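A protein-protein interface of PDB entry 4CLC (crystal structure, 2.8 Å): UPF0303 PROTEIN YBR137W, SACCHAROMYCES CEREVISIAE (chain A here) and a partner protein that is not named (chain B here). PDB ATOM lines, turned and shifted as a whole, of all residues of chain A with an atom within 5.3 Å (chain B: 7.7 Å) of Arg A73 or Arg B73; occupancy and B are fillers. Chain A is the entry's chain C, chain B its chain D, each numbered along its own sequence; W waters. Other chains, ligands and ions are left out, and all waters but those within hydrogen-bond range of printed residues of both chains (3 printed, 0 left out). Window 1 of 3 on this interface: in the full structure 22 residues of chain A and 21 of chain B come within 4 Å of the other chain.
N of Cys B70 is in hydrogen-bond range of OD2 of Asp A85. The backbone NH (N) of Cys A70 sits at hydrogen-bond distance from the side-chain carboxylate (OD2) of Asp B85 (3.1 Å). ND1 of His B69 sits at hydrogen-bond distance from OD1 of Asp A85 (2.8 Å). The backbone carbonyl oxygen of Arg A73 lies within hydrogen-bond range of the backbone NH of Arg B73, 3.0 Å away. O of Leu A71 sits at hydrogen-bond distance from N of Val B75.
The backbone NH (N) of Ile B63 is in hydrogen-bond range of the backbone carbonyl oxygen (O) of Phe B72 (3.0 Å). OD2 of Asp B62 sits at hydrogen-bond distance from SG of Cys B70, 3.5 Å away. OD2 of Asp B62 is in salt-bridge range of NE of Arg B73 (2.5 Å). The backbone carbonyl oxygen of Phe A72 lies within hydrogen-bond range of the side-chain sulfur of Cys A70 (3.7 Å). N of Ile B61 sits at hydrogen-bond distance from O of Thr B74. The backbone carbonyl oxygen (O) of Ile B63 is in hydrogen-bond range of the backbone NH (N) of Leu B71 (2.9 Å).
Among the printed residues, merely in contact across the chains: Leu A71 with Thr B74, Arg A73 with Phe B72, Thr A74 with Leu B71, Asp A85 with Gly B68, Phe A72 with Arg B73, Val A75 with Leu B71, Arg A73 with Cys B70, Thr A74 with Phe B40, Leu A71 with Arg B73, Arg A73 with Leu B71, Cys A70 with Arg B73 and Val A75 with His B69.
Printed residues of chain B within 4 Å of Leu A71: Arg B73, Thr B74 and Val B75. Of the printed residues of chain B, Arg A73 touches Cys B70, Leu B71, Phe B72 and Arg B73. Of the printed residues of chain A, Phe B40 touches Thr A74 (3.7 Å). Of the printed residues of chain A, Gly B68 touches Asp A85 (3.5 Å). Of the printed residues of chain A, Phe B72 touches Arg A73 (3.3 Å). Printed residues of chain A within 4 Å of Arg B73: Cys A70 (3.8 Å), Leu A71 (3.7 Å), Phe A72 (3.6 Å) and Arg A73 (3.0 Å). Printed residues of chain A within 4 Å of Val B75: Leu A71. The nearest printed residue of chain A that does not touch Phe B40 is Phe A72 (4.8 Å).
Hydrophobic or aromatic side chains of chain B that line the printed part of chain A: Phe B40 and His B69. Among the printed residues, 17 pairs touch across the chains. Among the printed residues, no Asp or Glu carboxylate lies within 4 Å of a Lys or Arg side-chain nitrogen of the other chain.
Water W2 lies within hydrogen-bond range of the side-chain hydroxyl of Thr B74 (2.4 Å) and the backbone carbonyl oxygen of Leu A71 (3.1 Å). Water W3 lies within hydrogen-bond range of NH1 of Arg A73, O of Cys B70 and OD1 of Asp A85. Water W1 lies within hydrogen-bond range of the side-chain hydroxyl of Thr A74, the backbone carbonyl oxygen of Leu B71 and the backbone carbonyl oxygen of Val A75.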
ATOM      1  N   ALA A  60     -14.176  15.348  21.082  1.00  0.00           N
ATOM      2  CA  ALA A  60     -13.959  16.162  19.894  1.00  0.00           C
ATOM      3  C   ALA A  60     -12.631  16.897  20.013  1.00  0.00           C
ATOM      4  O   ALA A  60     -12.335  17.477  21.049  1.00  0.00           O
ATOM      5  CB  ALA A  60     -15.105  17.128  19.702  1.00  0.00           C
ATOM      6  N   ILE A  61     -11.824  16.851  18.955  1.00  0.00           N
ATOM      7  CA  ILE A  61     -10.500  17.490  18.942  1.00  0.00           C
ATOM      8  C   ILE A  61     -10.460  18.595  17.888  1.00  0.00           C
ATOM      9  O   ILE A  61     -10.931  18.394  16.784  1.00  0.00           O
ATOM     10  CB  ILE A  61      -9.391  16.437  18.666  1.00  0.00           C
ATOM     11  CG1 ILE A  61      -9.379  15.395  19.779  1.00  0.00           C
ATOM     12  CG2 ILE A  61      -8.038  17.076  18.519  1.00  0.00           C
ATOM     13  CD1 ILE A  61      -9.026  14.023  19.306  1.00  0.00           C
ATOM     14  N   ASP A  62      -9.916  19.761  18.223  1.00  0.00           N
ATOM     15  CA  ASP A  62      -9.883  20.881  17.291  1.00  0.00           C
ATOM     16  C   ASP A  62      -8.534  21.574  17.240  1.00  0.00           C
ATOM     17  O   ASP A  62      -7.979  21.884  18.282  1.00  0.00           O
ATOM     18  CB  ASP A  62     -10.944  21.905  17.667  1.00  0.00           C
ATOM     19  CG  ASP A  62     -11.030  23.059  16.676  1.00  0.00           C
ATOM     20  OD1 ASP A  62     -10.300  24.049  16.849  1.00  0.00           O
ATOM     21  OD2 ASP A  62     -11.839  22.992  15.727  1.00  0.00           O
ATOM     22  N   ILE A  63      -8.011  21.840  16.041  1.00  0.00           N
ATOM     23  CA  ILE A  63      -6.874  22.747  15.920  1.00  0.00           C
ATOM     24  C   ILE A  63      -7.210  23.906  15.000  1.00  0.00           C
ATOM     25  O   ILE A  63      -7.522  23.697  13.843  1.00  0.00           O
ATOM     26  CB  ILE A  63      -5.617  22.045  15.398  1.00  0.00           C
ATOM     27  CG1 ILE A  63      -5.254  20.853  16.283  1.00  0.00           C
ATOM     28  CG2 ILE A  63      -4.450  23.021  15.361  1.00  0.00           C
ATOM     29  CD1 ILE A  63      -4.144  19.987  15.717  1.00  0.00           C
ATOM     30  N   CYS A  70     -10.096  26.868  10.809  1.00  0.00           N
ATOM     31  CA  CYS A  70     -10.011  25.546  11.382  1.00  0.00           C
ATOM     32  C   CYS A  70      -9.237  24.619  10.464  1.00  0.00           C
ATOM     33  O   CYS A  70      -9.583  24.466   9.291  1.00  0.00           O
ATOM     34  CB  CYS A  70     -11.404  24.996  11.655  1.00  0.00           C
ATOM     35  SG  CYS A  70     -11.421  23.275  12.185  1.00  0.00           S
ATOM     36  N   LEU A  71      -8.189  24.012  11.019  1.00  0.00           N
ATOM     37  CA  LEU A  71      -7.271  23.128  10.317  1.00  0.00           C
ATOM     38  C   LEU A  71      -7.656  21.673  10.492  1.00  0.00           C
ATOM     39  O   LEU A  71      -7.677  20.905   9.542  1.00  0.00           O
ATOM     40  CB  LEU A  71      -5.844  23.347  10.787  1.00  0.00           C
ATOM     41  CG  LEU A  71      -5.238  24.747  10.637  1.00  0.00           C
ATOM     42  CD1 LEU A  71      -3.769  24.727  11.044  1.00  0.00           C
ATOM     43  CD2 LEU A  71      -5.390  25.273   9.240  1.00  0.00           C
ATOM     44  N   PHE A  72      -7.803  21.250  11.734  1.00  0.00           N
ATOM     45  CA  PHE A  72      -8.174  19.870  12.013  1.00  0.00           C
ATOM     46  C   PHE A  72      -9.413  19.810  12.885  1.00  0.00           C
ATOM     47  O   PHE A  72      -9.546  20.588  13.818  1.00  0.00           O
ATOM     48  CB  PHE A  72      -7.010  19.139  12.697  1.00  0.00           C
ATOM     49  CG  PHE A  72      -7.305  17.715  13.027  1.00  0.00           C
ATOM     50  CD1 PHE A  72      -7.143  16.728  12.082  1.00  0.00           C
ATOM     51  CD2 PHE A  72      -7.756  17.361  14.281  1.00  0.00           C
ATOM     52  CE1 PHE A  72      -7.427  15.418  12.385  1.00  0.00           C
ATOM     53  CE2 PHE A  72      -8.040  16.048  14.575  1.00  0.00           C
ATOM     54  CZ  PHE A  72      -7.873  15.082  13.629  1.00  0.00           C
ATOM     55  N   ARG A  73     -10.339  18.918  12.577  1.00  0.00           N
ATOM     56  CA  ARG A  73     -11.353  18.591  13.554  1.00  0.00           C
ATOM     57  C   ARG A  73     -11.699  17.124  13.474  1.00  0.00           C
ATOM     58  O   ARG A  73     -11.949  16.609  12.404  1.00  0.00           O
ATOM     59  CB  ARG A  73     -12.608  19.424  13.360  1.00  0.00           C
ATOM     60  CG  ARG A  73     -13.783  18.939  14.219  1.00  0.00           C
ATOM     61  CD  ARG A  73     -13.670  19.433  15.656  1.00  0.00           C
ATOM     62  NE  ARG A  73     -13.541  20.880  15.692  1.00  0.00           N
ATOM     63  CZ  ARG A  73     -14.567  21.714  15.748  1.00  0.00           C
ATOM     64  NH1 ARG A  73     -15.805  21.250  15.805  1.00  0.00           N
ATOM     65  NH2 ARG A  73     -14.354  23.020  15.756  1.00  0.00           N
ATOM     66  N   THR A  74     -11.725  16.439  14.601  1.00  0.00           N
ATOM     67  CA  THR A  74     -12.239  15.091  14.576  1.00  0.00           C
ATOM     68  C   THR A  74     -13.102  14.774  15.794  1.00  0.00           C
ATOM     69  O   THR A  74     -13.291  15.587  16.682  1.00  0.00           O
ATOM     70  CB  THR A  74     -11.104  14.064  14.477  1.00  0.00           C
ATOM     71  OG1 THR A  74     -11.643  12.784  14.128  1.00  0.00           O
ATOM     72  CG2 THR A  74     -10.362  13.967  15.790  1.00  0.00           C
ATOM     73  N   VAL A  75     -13.627  13.569  15.803  1.00  0.00           N
ATOM     74  CA  VAL A  75     -14.514  13.111  16.838  1.00  0.00           C
ATOM     75  C   VAL A  75     -14.045  11.691  17.106  1.00  0.00           C
ATOM     76  O   VAL A  75     -13.899  10.899  16.175  1.00  0.00           O
ATOM     77  CB  VAL A  75     -16.014  13.218  16.387  1.00  0.00           C
ATOM     78  CG1 VAL A  75     -16.786  11.938  16.620  1.00  0.00           C
ATOM     79  CG2 VAL A  75     -16.701  14.402  17.063  1.00  0.00           C
ATOM     80  N   ASP A  85     -19.192  21.203  19.950  1.00  0.00           N
ATOM     81  CA  ASP A  85     -18.671  22.257  19.101  1.00  0.00           C
ATOM     82  C   ASP A  85     -18.765  23.567  19.847  1.00  0.00           C
ATOM     83  O   ASP A  85     -17.953  24.472  19.646  1.00  0.00           O
ATOM     84  CB  ASP A  85     -19.391  22.359  17.745  1.00  0.00           C
ATOM     85  CG  ASP A  85     -19.526  21.018  17.000  1.00  0.00           C
ATOM     86  OD1 ASP A  85     -19.205  19.920  17.508  1.00  0.00           O
ATOM     87  OD2 ASP A  85     -19.842  21.084  15.799  1.00  0.00           O
ATOM     88  N   ILE A  88     -15.974  23.626  22.303  1.00  0.00           N
ATOM     89  CA  ILE A  88     -14.738  23.878  21.578  1.00  0.00           C
ATOM     90  C   ILE A  88     -14.575  25.355  21.269  1.00  0.00           C
ATOM     91  O   ILE A  88     -13.510  25.899  21.507  1.00  0.00           O
ATOM     92  CB  ILE A  88     -14.640  23.056  20.283  1.00  0.00           C
ATOM     93  CG1 ILE A  88     -14.322  21.599  20.632  1.00  0.00           C
ATOM     94  CG2 ILE A  88     -13.531  23.592  19.405  1.00  0.00           C
ATOM     95  CD1 ILE A  88     -14.395  20.604  19.472  1.00  0.00           C
ATOM     96  N   GLN A  89     -15.628  26.017  20.791  1.00  0.00           N
ATOM     97  CA  GLN A  89     -15.523  27.441  20.463  1.00  0.00           C
ATOM     98  C   GLN A  89     -15.309  28.227  21.721  1.00  0.00           C
ATOM     99  O   GLN A  89     -14.466  29.110  21.803  1.00  0.00           O
ATOM    100  CB  GLN A  89     -16.774  27.953  19.733  1.00  0.00           C
ATOM    101  CG  GLN A  89     -16.858  27.474  18.283  1.00  0.00           C
ATOM    102  CD  GLN A  89     -15.526  27.619  17.515  1.00  0.00           C
ATOM    103  OE1 GLN A  89     -15.089  28.736  17.215  1.00  0.00           O
ATOM    104  NE2 GLN A  89     -14.880  26.484  17.209  1.00  0.00           N
ATOM    105  N   ALA B  39     -17.158   8.462   9.215  1.00  0.00           N
ATOM    106  CA  ALA B  39     -16.846   9.858   8.980  1.00  0.00           C
ATOM    107  C   ALA B  39     -15.356  10.036   8.785  1.00  0.00           C
ATOM    108  O   ALA B  39     -14.923  10.663   7.831  1.00  0.00           O
ATOM    109  CB  ALA B  39     -17.339  10.722  10.136  1.00  0.00           C
ATOM    110  N   PHE B  40     -14.568   9.475   9.689  1.00  0.00           N
ATOM    111  CA  PHE B  40     -13.140   9.726   9.665  1.00  0.00           C
ATOM    112  C   PHE B  40     -12.499   9.032   8.465  1.00  0.00           C
ATOM    113  O   PHE B  40     -11.594   9.573   7.813  1.00  0.00           O
ATOM    114  CB  PHE B  40     -12.486   9.263  10.966  1.00  0.00           C
ATOM    115  CG  PHE B  40     -11.009   9.533  11.015  1.00  0.00           C
ATOM    116  CD1 PHE B  40     -10.538  10.822  11.212  1.00  0.00           C
ATOM    117  CD2 PHE B  40     -10.092   8.501  10.836  1.00  0.00           C
ATOM    118  CE1 PHE B  40      -9.186  11.086  11.251  1.00  0.00           C
ATOM    119  CE2 PHE B  40      -8.741   8.756  10.864  1.00  0.00           C
ATOM    120  CZ  PHE B  40      -8.280  10.053  11.080  1.00  0.00           C
ATOM    121  N   GLY B  43     -13.500  11.054   5.353  1.00  0.00           N
ATOM    122  CA  GLY B  43     -12.785  12.310   5.271  1.00  0.00           C
ATOM    123  C   GLY B  43     -11.329  12.172   4.852  1.00  0.00           C
ATOM    124  O   GLY B  43     -10.809  13.022   4.121  1.00  0.00           O
ATOM    125  N   ARG B  47      -9.333  13.190   1.531  1.00  0.00           N
ATOM    126  CA  ARG B  47      -8.182  14.049   1.742  1.00  0.00           C
ATOM    127  C   ARG B  47      -7.064  13.527   0.875  1.00  0.00           C
ATOM    128  O   ARG B  47      -6.353  14.301   0.232  1.00  0.00           O
ATOM    129  CB  ARG B  47      -7.756  14.100   3.214  1.00  0.00           C
ATOM    130  CG  ARG B  47      -6.606  15.088   3.471  1.00  0.00           C
ATOM    131  CD  ARG B  47      -6.151  15.058   4.913  1.00  0.00           C
ATOM    132  NE  ARG B  47      -5.018  15.942   5.132  1.00  0.00           N
ATOM    133  CZ  ARG B  47      -3.762  15.572   4.943  1.00  0.00           C
ATOM    134  NH1 ARG B  47      -3.510  14.339   4.522  1.00  0.00           N
ATOM    135  NH2 ARG B  47      -2.763  16.421   5.157  1.00  0.00           N
ATOM    136  N   VAL B  59      -7.121  22.830  -0.132  1.00  0.00           N
ATOM    137  CA  VAL B  59      -8.534  22.530  -0.200  1.00  0.00           C
ATOM    138  C   VAL B  59      -9.052  22.187   1.182  1.00  0.00           C
ATOM    139  O   VAL B  59      -8.364  21.530   1.956  1.00  0.00           O
ATOM    140  CB  VAL B  59      -8.802  21.387  -1.195  1.00  0.00           C
ATOM    141  CG1 VAL B  59     -10.188  20.846  -1.046  1.00  0.00           C
ATOM    142  CG2 VAL B  59      -8.603  21.887  -2.591  1.00  0.00           C
ATOM    143  N   ALA B  60     -10.253  22.668   1.494  1.00  0.00           N
ATOM    144  CA  ALA B  60     -10.861  22.429   2.790  1.00  0.00           C
ATOM    145  C   ALA B  60     -11.946  21.372   2.631  1.00  0.00           C
ATOM    146  O   ALA B  60     -12.694  21.393   1.670  1.00  0.00           O
ATOM    147  CB  ALA B  60     -11.412  23.711   3.370  1.00  0.00           C
ATOM    148  N   ILE B  61     -12.006  20.437   3.568  1.00  0.00           N
ATOM    149  CA  ILE B  61     -12.946  19.334   3.508  1.00  0.00           C
ATOM    150  C   ILE B  61     -13.751  19.241   4.800  1.00  0.00           C
ATOM    151  O   ILE B  61     -13.165  19.155   5.865  1.00  0.00           O
ATOM    152  CB  ILE B  61     -12.207  18.003   3.263  1.00  0.00           C
ATOM    153  CG1 ILE B  61     -11.438  18.060   1.946  1.00  0.00           C
ATOM    154  CG2 ILE B  61     -13.166  16.839   3.279  1.00  0.00           C
ATOM    155  CD1 ILE B  61     -10.456  16.937   1.784  1.00  0.00           C
ATOM    156  N   ASP B  62     -15.082  19.251   4.714  1.00  0.00           N
ATOM    157  CA  ASP B  62     -15.913  19.157   5.907  1.00  0.00           C
ATOM    158  C   ASP B  62     -16.898  17.968   5.884  1.00  0.00           C
ATOM    159  O   ASP B  62     -17.430  17.590   4.837  1.00  0.00           O
ATOM    160  CB  ASP B  62     -16.684  20.469   6.111  1.00  0.00           C
ATOM    161  CG  ASP B  62     -17.420  20.522   7.458  1.00  0.00           C
ATOM    162  OD1 ASP B  62     -18.590  20.081   7.523  1.00  0.00           O
ATOM    163  OD2 ASP B  62     -16.825  21.022   8.448  1.00  0.00           O
ATOM    164  N   ILE B  63     -17.140  17.370   7.041  1.00  0.00           N
ATOM    165  CA  ILE B  63     -18.281  16.475   7.172  1.00  0.00           C
ATOM    166  C   ILE B  63     -19.028  16.896   8.420  1.00  0.00           C
ATOM    167  O   ILE B  63     -18.468  16.863   9.512  1.00  0.00           O
ATOM    168  CB  ILE B  63     -17.874  14.987   7.262  1.00  0.00           C
ATOM    169  CG1 ILE B  63     -17.103  14.575   6.010  1.00  0.00           C
ATOM    170  CG2 ILE B  63     -19.101  14.094   7.455  1.00  0.00           C
ATOM    171  CD1 ILE B  63     -16.592  13.158   6.057  1.00  0.00           C
ATOM    172  N   SER B  64     -20.280  17.320   8.257  1.00  0.00           N
ATOM    173  CA  SER B  64     -21.075  17.768   9.380  1.00  0.00           C
ATOM    174  C   SER B  64     -22.439  17.112   9.353  1.00  0.00           C
ATOM    175  O   SER B  64     -22.887  16.625   8.326  1.00  0.00           O
ATOM    176  CB  SER B  64     -21.221  19.288   9.369  1.00  0.00           C
ATOM    177  OG  SER B  64     -19.974  19.937   9.552  1.00  0.00           O
ATOM    178  N   GLY B  68     -25.430  20.695  12.433  1.00  0.00           N
ATOM    179  CA  GLY B  68     -24.275  21.581  12.458  1.00  0.00           C
ATOM    180  C   GLY B  68     -23.039  20.981  13.106  1.00  0.00           C
ATOM    181  O   GLY B  68     -21.934  21.515  12.982  1.00  0.00           O
ATOM    182  N   HIS B  69     -23.241  19.861  13.799  1.00  0.00           N
ATOM    183  CA  HIS B  69     -22.160  19.157  14.482  1.00  0.00           C
ATOM    184  C   HIS B  69     -21.074  18.691  13.493  1.00  0.00           C
ATOM    185  O   HIS B  69     -21.335  17.908  12.583  1.00  0.00           O
ATOM    186  CB  HIS B  69     -22.730  17.960  15.272  1.00  0.00           C
ATOM    187  CG  HIS B  69     -21.682  17.136  15.958  1.00  0.00           C
ATOM    188  ND1 HIS B  69     -20.527  17.680  16.478  1.00  0.00           N
ATOM    189  CD2 HIS B  69     -21.611  15.802  16.197  1.00  0.00           C
ATOM    190  CE1 HIS B  69     -19.789  16.723  17.009  1.00  0.00           C
ATOM    191  NE2 HIS B  69     -20.425  15.574  16.858  1.00  0.00           N
ATOM    192  N   CYS B  70     -19.843  19.135  13.716  1.00  0.00           N
ATOM    193  CA  CYS B  70     -18.750  18.805  12.819  1.00  0.00           C
ATOM    194  C   CYS B  70     -18.096  17.493  13.234  1.00  0.00           C
ATOM    195  O   CYS B  70     -17.625  17.375  14.352  1.00  0.00           O
ATOM    196  CB  CYS B  70     -17.733  19.936  12.803  1.00  0.00           C
ATOM    197  SG  CYS B  70     -16.352  19.685  11.701  1.00  0.00           S
ATOM    198  N   LEU B  71     -18.149  16.487  12.370  1.00  0.00           N
ATOM    199  CA  LEU B  71     -17.447  15.231  12.601  1.00  0.00           C
ATOM    200  C   LEU B  71     -15.987  15.282  12.125  1.00  0.00           C
ATOM    201  O   LEU B  71     -15.100  14.681  12.734  1.00  0.00           O
ATOM    202  CB  LEU B  71     -18.194  14.086  11.930  1.00  0.00           C
ATOM    203  CG  LEU B  71     -19.682  14.041  12.286  1.00  0.00           C
ATOM    204  CD1 LEU B  71     -20.406  12.937  11.552  1.00  0.00           C
ATOM    205  CD2 LEU B  71     -19.888  13.874  13.773  1.00  0.00           C
ATOM    206  N   PHE B  72     -15.759  15.988  11.018  1.00  0.00           N
ATOM    207  CA  PHE B  72     -14.468  15.975  10.326  1.00  0.00           C
ATOM    208  C   PHE B  72     -14.143  17.281   9.677  1.00  0.00           C
ATOM    209  O   PHE B  72     -14.991  17.884   9.045  1.00  0.00           O
ATOM    210  CB  PHE B  72     -14.429  14.902   9.230  1.00  0.00           C
ATOM    211  CG  PHE B  72     -13.079  14.751   8.591  1.00  0.00           C
ATOM    212  CD1 PHE B  72     -12.134  13.916   9.141  1.00  0.00           C
ATOM    213  CD2 PHE B  72     -12.751  15.454   7.449  1.00  0.00           C
ATOM    214  CE1 PHE B  72     -10.882  13.784   8.565  1.00  0.00           C
ATOM    215  CE2 PHE B  72     -11.501  15.321   6.861  1.00  0.00           C
ATOM    216  CZ  PHE B  72     -10.568  14.485   7.429  1.00  0.00           C
ATOM    217  N   ARG B  73     -12.896  17.699   9.788  1.00  0.00           N
ATOM    218  CA  ARG B  73     -12.435  18.846   9.028  1.00  0.00           C
ATOM    219  C   ARG B  73     -10.944  18.703   8.770  1.00  0.00           C
ATOM    220  O   ARG B  73     -10.211  18.202   9.624  1.00  0.00           O
ATOM    221  CB  ARG B  73     -12.744  20.145   9.767  1.00  0.00           C
ATOM    222  CG  ARG B  73     -12.265  21.375   9.050  1.00  0.00           C
ATOM    223  CD  ARG B  73     -13.153  21.704   7.863  1.00  0.00           C
ATOM    224  NE  ARG B  73     -14.514  22.071   8.267  1.00  0.00           N
ATOM    225  CZ  ARG B  73     -14.857  23.277   8.706  1.00  0.00           C
ATOM    226  NH1 ARG B  73     -13.943  24.233   8.813  1.00  0.00           N
ATOM    227  NH2 ARG B  73     -16.116  23.517   9.042  1.00  0.00           N
ATOM    228  N   THR B  74     -10.499  19.118   7.593  1.00  0.00           N
ATOM    229  CA  THR B  74      -9.075  19.126   7.300  1.00  0.00           C
ATOM    230  C   THR B  74      -8.739  20.127   6.217  1.00  0.00           C
ATOM    231  O   THR B  74      -9.599  20.656   5.540  1.00  0.00           O
ATOM    232  CB  THR B  74      -8.535  17.741   6.875  1.00  0.00           C
ATOM    233  OG1 THR B  74      -7.111  17.796   6.824  1.00  0.00           O
ATOM    234  CG2 THR B  74      -9.045  17.353   5.520  1.00  0.00           C
ATOM    235  N   VAL B  75      -7.460  20.401   6.089  1.00  0.00           N
ATOM    236  CA  VAL B  75      -6.972  21.346   5.127  1.00  0.00           C
ATOM    237  C   VAL B  75      -5.925  20.563   4.317  1.00  0.00           C
ATOM    238  O   VAL B  75      -5.068  19.908   4.912  1.00  0.00           O
ATOM    239  CB  VAL B  75      -6.434  22.600   5.871  1.00  0.00           C
ATOM    240  CG1 VAL B  75      -5.076  23.038   5.375  1.00  0.00           C
ATOM    241  CG2 VAL B  75      -7.447  23.720   5.817  1.00  0.00           C
ATOM    242  N   ASN B  84     -12.229  29.907   3.546  1.00  0.00           N
ATOM    243  CA  ASN B  84     -12.511  28.518   3.254  1.00  0.00           C
ATOM    244  C   ASN B  84     -13.604  28.056   4.192  1.00  0.00           C
ATOM    245  O   ASN B  84     -14.453  27.252   3.833  1.00  0.00           O
ATOM    246  CB  ASN B  84     -11.284  27.637   3.401  1.00  0.00           C
ATOM    247  CG  ASN B  84     -10.373  27.712   2.207  1.00  0.00           C
ATOM    248  OD1 ASN B  84      -9.227  28.139   2.320  1.00  0.00           O
ATOM    249  ND2 ASN B  84     -10.874  27.290   1.049  1.00  0.00           N
ATOM    250  N   ASP B  85     -13.584  28.596   5.405  1.00  0.00           N
ATOM    251  CA  ASP B  85     -14.574  28.237   6.413  1.00  0.00           C
ATOM    252  C   ASP B  85     -15.922  28.874   6.092  1.00  0.00           C
ATOM    253  O   ASP B  85     -16.966  28.214   6.170  1.00  0.00           O
ATOM    254  CB  ASP B  85     -14.097  28.648   7.807  1.00  0.00           C
ATOM    255  CG  ASP B  85     -12.907  27.840   8.279  1.00  0.00           C
ATOM    256  OD1 ASP B  85     -12.726  26.676   7.850  1.00  0.00           O
ATOM    257  OD2 ASP B  85     -12.126  28.371   9.078  1.00  0.00           O
ATOM    258  N   PHE B  86     -15.894  30.150   5.727  1.00  0.00           N
ATOM    259  CA  PHE B  86     -17.093  30.824   5.271  1.00  0.00           C
ATOM    260  C   PHE B  86     -17.734  30.072   4.094  1.00  0.00           C
ATOM    261  O   PHE B  86     -18.937  29.800   4.105  1.00  0.00           O
ATOM    262  CB  PHE B  86     -16.768  32.257   4.878  1.00  0.00           C
ATOM    263  CG  PHE B  86     -16.543  33.163   6.042  1.00  0.00           C
ATOM    264  CD1 PHE B  86     -17.620  33.786   6.669  1.00  0.00           C
ATOM    265  CD2 PHE B  86     -15.256  33.400   6.520  1.00  0.00           C
ATOM    266  CE1 PHE B  86     -17.434  34.623   7.753  1.00  0.00           C
ATOM    267  CE2 PHE B  86     -15.051  34.247   7.606  1.00  0.00           C
ATOM    268  CZ  PHE B  86     -16.159  34.859   8.222  1.00  0.00           C
ATOM    269  N   ILE B  88     -17.321  26.993   3.213  1.00  0.00           N
ATOM    270  CA  ILE B  88     -17.824  25.719   3.692  1.00  0.00           C
ATOM    271  C   ILE B  88     -19.170  25.892   4.393  1.00  0.00           C
ATOM    272  O   ILE B  88     -20.088  25.115   4.156  1.00  0.00           O
ATOM    273  CB  ILE B  88     -16.817  25.038   4.626  1.00  0.00           C
ATOM    274  CG1 ILE B  88     -15.677  24.458   3.794  1.00  0.00           C
ATOM    275  CG2 ILE B  88     -17.489  23.912   5.433  1.00  0.00           C
ATOM    276  CD1 ILE B  88     -14.734  23.633   4.590  1.00  0.00           C
ATOM    277  N   GLN B  89     -19.291  26.926   5.224  1.00  0.00           N
ATOM    278  CA  GLN B  89     -20.529  27.153   5.956  1.00  0.00           C
ATOM    279  C   GLN B  89     -21.641  27.552   5.019  1.00  0.00           C
ATOM    280  O   GLN B  89     -22.748  27.022   5.086  1.00  0.00           O
ATOM    281  CB  GLN B  89     -20.345  28.220   7.025  1.00  0.00           C
ATOM    282  CG  GLN B  89     -21.070  27.880   8.320  1.00  0.00           C
ATOM    283  CD  GLN B  89     -20.563  26.575   8.972  1.00  0.00           C
ATOM    284  OE1 GLN B  89     -19.548  25.989   8.556  1.00  0.00           O
ATOM    285  NE2 GLN B  89     -21.271  26.129  10.012  1.00  0.00           N
ATOM    286  N   LYS B  92     -22.665  24.458   2.672  1.00  0.00           N
ATOM    287  CA  LYS B  92     -23.346  23.482   3.520  1.00  0.00           C
ATOM    288  C   LYS B  92     -24.742  23.961   3.851  1.00  0.00           C
ATOM    289  O   LYS B  92     -25.702  23.194   3.798  1.00  0.00           O
ATOM    290  CB  LYS B  92     -22.546  23.247   4.812  1.00  0.00           C
ATOM    291  CG  LYS B  92     -23.160  22.246   5.757  1.00  0.00           C
ATOM    292  CD  LYS B  92     -22.318  22.003   6.991  1.00  0.00           C
ATOM    293  CE  LYS B  92     -22.057  23.257   7.756  1.00  0.00           C
ATOM    294  NZ  LYS B  92     -20.590  23.468   7.848  1.00  0.00           N
ATOM    295  N   THR B 147     -18.649  18.697   2.275  1.00  0.00           N
ATOM    296  CA  THR B 147     -18.408  19.988   1.660  1.00  0.00           C
ATOM    297  C   THR B 147     -16.936  20.216   1.388  1.00  0.00           C
ATOM    298  O   THR B 147     -16.109  20.143   2.298  1.00  0.00           O
ATOM    299  CB  THR B 147     -18.908  21.144   2.525  1.00  0.00           C
ATOM    300  OG1 THR B 147     -20.303  20.996   2.788  1.00  0.00           O
ATOM    301  CG2 THR B 147     -18.673  22.451   1.814  1.00  0.00           C
HETATM  302  O   HOH W   1     -14.047  11.488  12.838  1.00  0.00           O
HETATM  303  O   HOH W   2      -5.852  18.519   8.781  1.00  0.00           O
HETATM  304  O   HOH W   3     -16.803  18.973  16.175  1.00  0.00           O
